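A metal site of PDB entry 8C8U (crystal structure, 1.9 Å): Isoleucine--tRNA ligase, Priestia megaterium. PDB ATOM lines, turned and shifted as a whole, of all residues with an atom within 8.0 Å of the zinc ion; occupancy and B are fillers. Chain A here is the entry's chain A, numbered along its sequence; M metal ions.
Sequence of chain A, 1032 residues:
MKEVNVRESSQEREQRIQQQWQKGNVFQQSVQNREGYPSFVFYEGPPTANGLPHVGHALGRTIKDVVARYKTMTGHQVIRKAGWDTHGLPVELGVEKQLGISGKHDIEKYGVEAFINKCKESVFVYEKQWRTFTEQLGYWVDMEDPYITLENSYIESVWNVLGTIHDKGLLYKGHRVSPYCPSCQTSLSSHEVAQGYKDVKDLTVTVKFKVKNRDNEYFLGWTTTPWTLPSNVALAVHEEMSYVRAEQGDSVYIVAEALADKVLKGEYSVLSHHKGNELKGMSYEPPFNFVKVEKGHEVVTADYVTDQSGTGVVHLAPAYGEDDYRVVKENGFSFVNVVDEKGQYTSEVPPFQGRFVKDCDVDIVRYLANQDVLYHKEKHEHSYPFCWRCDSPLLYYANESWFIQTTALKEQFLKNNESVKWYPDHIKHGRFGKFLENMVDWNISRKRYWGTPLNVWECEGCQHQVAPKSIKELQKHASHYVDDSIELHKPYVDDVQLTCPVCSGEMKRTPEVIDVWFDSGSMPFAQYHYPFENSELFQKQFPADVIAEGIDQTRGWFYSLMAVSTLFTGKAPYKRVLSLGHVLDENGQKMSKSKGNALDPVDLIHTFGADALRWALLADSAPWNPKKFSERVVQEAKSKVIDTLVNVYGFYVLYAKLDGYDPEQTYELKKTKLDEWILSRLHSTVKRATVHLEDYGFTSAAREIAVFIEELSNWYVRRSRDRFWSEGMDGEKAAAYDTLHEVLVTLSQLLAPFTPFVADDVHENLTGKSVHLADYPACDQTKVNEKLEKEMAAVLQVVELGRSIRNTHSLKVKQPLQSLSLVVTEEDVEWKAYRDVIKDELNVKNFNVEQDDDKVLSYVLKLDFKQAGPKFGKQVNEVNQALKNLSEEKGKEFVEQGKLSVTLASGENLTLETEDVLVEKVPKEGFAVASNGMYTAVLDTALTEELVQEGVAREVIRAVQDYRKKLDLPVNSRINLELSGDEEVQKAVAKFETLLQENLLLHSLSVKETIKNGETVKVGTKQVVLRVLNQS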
ATOM      1  N   GLU A 458     -17.080 -22.511 -21.716  1.00  0.00           N
ATOM      2  CA  GLU A 458     -17.892 -22.676 -20.508  1.00  0.00           C
ATOM      3  C   GLU A 458     -19.365 -22.882 -20.872  1.00  0.00           C
ATOM      4  O   GLU A 458     -19.926 -22.075 -21.614  1.00  0.00           O
ATOM      5  CB  GLU A 458     -17.791 -21.461 -19.591  1.00  0.00           C
ATOM      6  CG  GLU A 458     -16.419 -21.208 -18.979  1.00  0.00           C
ATOM      7  CD  GLU A 458     -16.344 -19.858 -18.308  1.00  0.00           C
ATOM      8  OE1 GLU A 458     -16.203 -18.844 -19.027  1.00  0.00           O
ATOM      9  OE2 GLU A 458     -16.448 -19.794 -17.058  1.00  0.00           O
ATOM     10  N   CYS A 459     -19.973 -23.928 -20.317  1.00  0.00           N
ATOM     11  CA  CYS A 459     -21.381 -24.235 -20.581  1.00  0.00           C
ATOM     12  C   CYS A 459     -22.289 -23.153 -19.993  1.00  0.00           C
ATOM     13  O   CYS A 459     -22.225 -22.869 -18.804  1.00  0.00           O
ATOM     14  CB  CYS A 459     -21.742 -25.598 -19.997  1.00  0.00           C
ATOM     15  SG  CYS A 459     -23.558 -25.994 -20.031  1.00  0.00           S
ATOM     16  N   GLU A 460     -23.156 -22.565 -20.835  1.00  0.00           N
ATOM     17  CA  GLU A 460     -24.069 -21.537 -20.338  1.00  0.00           C
ATOM     18  C   GLU A 460     -25.069 -22.093 -19.332  1.00  0.00           C
ATOM     19  O   GLU A 460     -25.609 -21.338 -18.531  1.00  0.00           O
ATOM     20  CB  GLU A 460     -24.808 -20.861 -21.501  1.00  0.00           C
ATOM     21  CG  GLU A 460     -25.863 -21.738 -22.171  1.00  0.00           C
ATOM     22  CD  GLU A 460     -26.484 -21.106 -23.413  1.00  0.00           C
ATOM     23  OE1 GLU A 460     -26.226 -19.914 -23.691  1.00  0.00           O
ATOM     24  OE2 GLU A 460     -27.237 -21.823 -24.124  1.00  0.00           O
ATOM     25  N   GLY A 461     -25.316 -23.408 -19.361  1.00  0.00           N
ATOM     26  CA  GLY A 461     -26.188 -24.037 -18.395  1.00  0.00           C
ATOM     27  C   GLY A 461     -25.579 -24.211 -17.012  1.00  0.00           C
ATOM     28  O   GLY A 461     -26.081 -23.643 -16.038  1.00  0.00           O
ATOM     29  N   CYS A 462     -24.485 -24.972 -16.924  1.00  0.00           N
ATOM     30  CA  CYS A 462     -23.934 -25.373 -15.627  1.00  0.00           C
ATOM     31  C   CYS A 462     -22.506 -24.883 -15.383  1.00  0.00           C
ATOM     32  O   CYS A 462     -21.912 -25.266 -14.365  1.00  0.00           O
ATOM     33  CB  CYS A 462     -23.969 -26.891 -15.498  1.00  0.00           C
ATOM     34  SG  CYS A 462     -22.845 -27.721 -16.629  1.00  0.00           S
ATOM     35  N   GLN A 463     -21.940 -24.059 -16.259  1.00  0.00           N
ATOM     36  CA  GLN A 463     -20.617 -23.465 -16.130  1.00  0.00           C
ATOM     37  C   GLN A 463     -19.479 -24.475 -16.255  1.00  0.00           C
ATOM     38  O   GLN A 463     -18.324 -24.088 -16.053  1.00  0.00           O
ATOM     39  CB  GLN A 463     -20.441 -22.691 -14.807  1.00  0.00           C
ATOM     40  CG  GLN A 463     -21.314 -21.451 -14.656  1.00  0.00           C
ATOM     41  CD  GLN A 463     -22.733 -21.787 -14.231  1.00  0.00           C
ATOM     42  OE1 GLN A 463     -22.954 -22.494 -13.241  1.00  0.00           O
ATOM     43  NE2 GLN A 463     -23.718 -21.291 -14.987  1.00  0.00           N
ATOM     44  N   HIS A 464     -19.761 -25.741 -16.570  1.00  0.00           N
ATOM     45  CA  HIS A 464     -18.708 -26.714 -16.844  1.00  0.00           C
ATOM     46  C   HIS A 464     -17.725 -26.187 -17.898  1.00  0.00           C
ATOM     47  O   HIS A 464     -18.106 -25.414 -18.778  1.00  0.00           O
ATOM     48  CB  HIS A 464     -19.338 -28.023 -17.321  1.00  0.00           C
ATOM     49  CG  HIS A 464     -18.352 -29.131 -17.547  1.00  0.00           C
ATOM     50  ND1 HIS A 464     -17.615 -29.694 -16.524  1.00  0.00           N
ATOM     51  CD2 HIS A 464     -18.016 -29.802 -18.670  1.00  0.00           C
ATOM     52  CE1 HIS A 464     -16.849 -30.650 -17.018  1.00  0.00           C
ATOM     53  NE2 HIS A 464     -17.074 -30.738 -18.321  1.00  0.00           N
ATOM     54  N   GLN A 465     -16.448 -26.594 -17.780  1.00  0.00           N
ATOM     55  CA  GLN A 465     -15.363 -26.125 -18.628  1.00  0.00           C
ATOM     56  C   GLN A 465     -14.834 -27.265 -19.505  1.00  0.00           C
ATOM     57  O   GLN A 465     -14.569 -28.362 -19.009  1.00  0.00           O
ATOM     58  CB  GLN A 465     -14.211 -25.541 -17.796  1.00  0.00           C
ATOM     59  CG  GLN A 465     -14.506 -24.216 -17.111  1.00  0.00           C
ATOM     60  CD  GLN A 465     -13.454 -23.841 -16.086  1.00  0.00           C
ATOM     61  OE1 GLN A 465     -12.307 -24.294 -16.162  1.00  0.00           O
ATOM     62  NE2 GLN A 465     -13.839 -23.034 -15.105  1.00  0.00           N
ATOM     63  N   THR A 499     -20.915 -28.646 -27.362  1.00  0.00           N
ATOM     64  CA  THR A 499     -21.945 -29.367 -26.638  1.00  0.00           C
ATOM     65  C   THR A 499     -21.394 -29.763 -25.280  1.00  0.00           C
ATOM     66  O   THR A 499     -20.393 -30.494 -25.208  1.00  0.00           O
ATOM     67  CB  THR A 499     -22.395 -30.588 -27.423  1.00  0.00           C
ATOM     68  OG1 THR A 499     -22.996 -30.169 -28.651  1.00  0.00           O
ATOM     69  CG2 THR A 499     -23.397 -31.458 -26.615  1.00  0.00           C
ATOM     70  N   CYS A 500     -22.019 -29.295 -24.220  1.00  0.00           N
ATOM     71  CA  CYS A 500     -21.545 -29.560 -22.859  1.00  0.00           C
ATOM     72  C   CYS A 500     -21.637 -31.044 -22.539  1.00  0.00           C
ATOM     73  O   CYS A 500     -22.732 -31.614 -22.611  1.00  0.00           O
ATOM     74  CB  CYS A 500     -22.346 -28.779 -21.837  1.00  0.00           C
ATOM     75  SG  CYS A 500     -22.034 -29.344 -20.164  1.00  0.00           S
ATOM     76  N   PRO A 501     -20.536 -31.713 -22.208  1.00  0.00           N
ATOM     77  CA  PRO A 501     -20.604 -33.157 -21.931  1.00  0.00           C
ATOM     78  C   PRO A 501     -21.412 -33.509 -20.687  1.00  0.00           C
ATOM     79  O   PRO A 501     -21.793 -34.671 -20.531  1.00  0.00           O
ATOM     80  CB  PRO A 501     -19.133 -33.566 -21.770  1.00  0.00           C
ATOM     81  CG  PRO A 501     -18.429 -32.284 -21.415  1.00  0.00           C
ATOM     82  CD  PRO A 501     -19.158 -31.189 -22.127  1.00  0.00           C
ATOM     83  N   VAL A 502     -21.644 -32.548 -19.796  1.00  0.00           N
ATOM     84  CA  VAL A 502     -22.429 -32.809 -18.594  1.00  0.00           C
ATOM     85  C   VAL A 502     -23.913 -32.790 -18.901  1.00  0.00           C
ATOM     86  O   VAL A 502     -24.623 -33.794 -18.704  1.00  0.00           O
ATOM     87  CB  VAL A 502     -22.065 -31.785 -17.506  1.00  0.00           C
ATOM     88  CG1 VAL A 502     -22.864 -32.029 -16.241  1.00  0.00           C
ATOM     89  CG2 VAL A 502     -20.586 -31.862 -17.199  1.00  0.00           C
ATOM     90  N   CYS A 503     -24.422 -31.664 -19.402  1.00  0.00           N
ATOM     91  CA  CYS A 503     -25.842 -31.469 -19.584  1.00  0.00           C
ATOM     92  C   CYS A 503     -26.259 -31.292 -21.036  1.00  0.00           C
ATOM     93  O   CYS A 503     -27.448 -31.075 -21.292  1.00  0.00           O
ATOM     94  CB  CYS A 503     -26.313 -30.253 -18.775  1.00  0.00           C
ATOM     95  SG  CYS A 503     -25.751 -28.672 -19.445  1.00  0.00           S
ATOM     96  N   SER A 504     -25.328 -31.378 -21.983  1.00  0.00           N
ATOM     97  CA  SER A 504     -25.570 -31.191 -23.420  1.00  0.00           C
ATOM     98  C   SER A 504     -26.048 -29.774 -23.758  1.00  0.00           C
ATOM     99  O   SER A 504     -26.519 -29.540 -24.877  1.00  0.00           O
ATOM    100  CB  SER A 504     -26.517 -32.250 -23.978  1.00  0.00           C
ATOM    101  OG  SER A 504     -27.722 -32.317 -23.236  1.00  0.00           O
ATOM    102  N   GLY A 505     -25.911 -28.797 -22.840  1.00  0.00           N
ATOM    103  CA  GLY A 505     -26.153 -27.417 -23.183  1.00  0.00           C
ATOM    104  C   GLY A 505     -25.031 -26.799 -24.024  1.00  0.00           C
ATOM    105  O   GLY A 505     -24.001 -27.419 -24.288  1.00  0.00           O
ATOM    106  N   GLU A 506     -25.238 -25.553 -24.466  1.00  0.00           N
ATOM    107  CA  GLU A 506     -24.262 -24.879 -25.305  1.00  0.00           C
ATOM    108  C   GLU A 506     -23.119 -24.289 -24.481  1.00  0.00           C
ATOM    109  O   GLU A 506     -23.349 -23.618 -23.475  1.00  0.00           O
ATOM    110  CB  GLU A 506     -24.921 -23.769 -26.117  1.00  0.00           C
ATOM    111  CG  GLU A 506     -25.876 -24.258 -27.189  1.00  0.00           C
ATOM    112  CD  GLU A 506     -25.183 -25.065 -28.286  1.00  0.00           C
ATOM    113  OE1 GLU A 506     -24.346 -24.492 -29.046  1.00  0.00           O
ATOM    114  OE2 GLU A 506     -25.476 -26.268 -28.417  1.00  0.00           O
ATOM    115  N   MET A 507     -21.890 -24.523 -24.919  1.00  0.00           N
ATOM    116  CA  MET A 507     -20.699 -23.939 -24.314  1.00  0.00           C
ATOM    117  C   MET A 507     -20.186 -22.814 -25.198  1.00  0.00           C
ATOM    118  O   MET A 507     -20.150 -22.939 -26.429  1.00  0.00           O
ATOM    119  CB  MET A 507     -19.590 -24.987 -24.123  1.00  0.00           C
ATOM    120  CG  MET A 507     -20.041 -26.284 -23.545  1.00  0.00           C
ATOM    121  SD  MET A 507     -18.678 -27.430 -23.200  1.00  0.00           S
ATOM    122  CE  MET A 507     -18.083 -26.697 -21.666  1.00  0.00           C
HETATM  123 ZN    ZN M   1     -23.456 -28.053 -18.961  1.00  0.00          ZN
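SG of Cys 500 binds the zinc ion, at 2.3 Å.
SG of Cys 459 is bound to the zinc ion.
SG of Cys 503 is bound to the zinc ion.
SG of Cys 462 binds the zinc ion, at 2.4 Å.
The zinc ion has four donor atoms within binding distance.
The side-chain sulfur (SG) of Cys 500 sits close to the backbone NH (N) of Val 502, 3.2 Å away.
O of Gly 505 is in hydrogen-bond range of N of Cys 500 (2.7 Å).
N of Cys 459 is in hydrogen-bond range of O of His 464.
The side-chain sulfur (SG) of Cys 459 sits close to the backbone NH (N) of Gly 461, 3.2 Å away.
N of Gly 505 lies close to SG of Cys 503, 3.4 Å away.
SG of Cys 462 lies close to N of His 464 (3.7 Å).
Within 4 Å of the zinc ion: Cys 459, Cys 462, Cys 500 and Cys 503.
The nearest printed residue that does not touch the zinc ion is Val 502 (4.2 Å).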
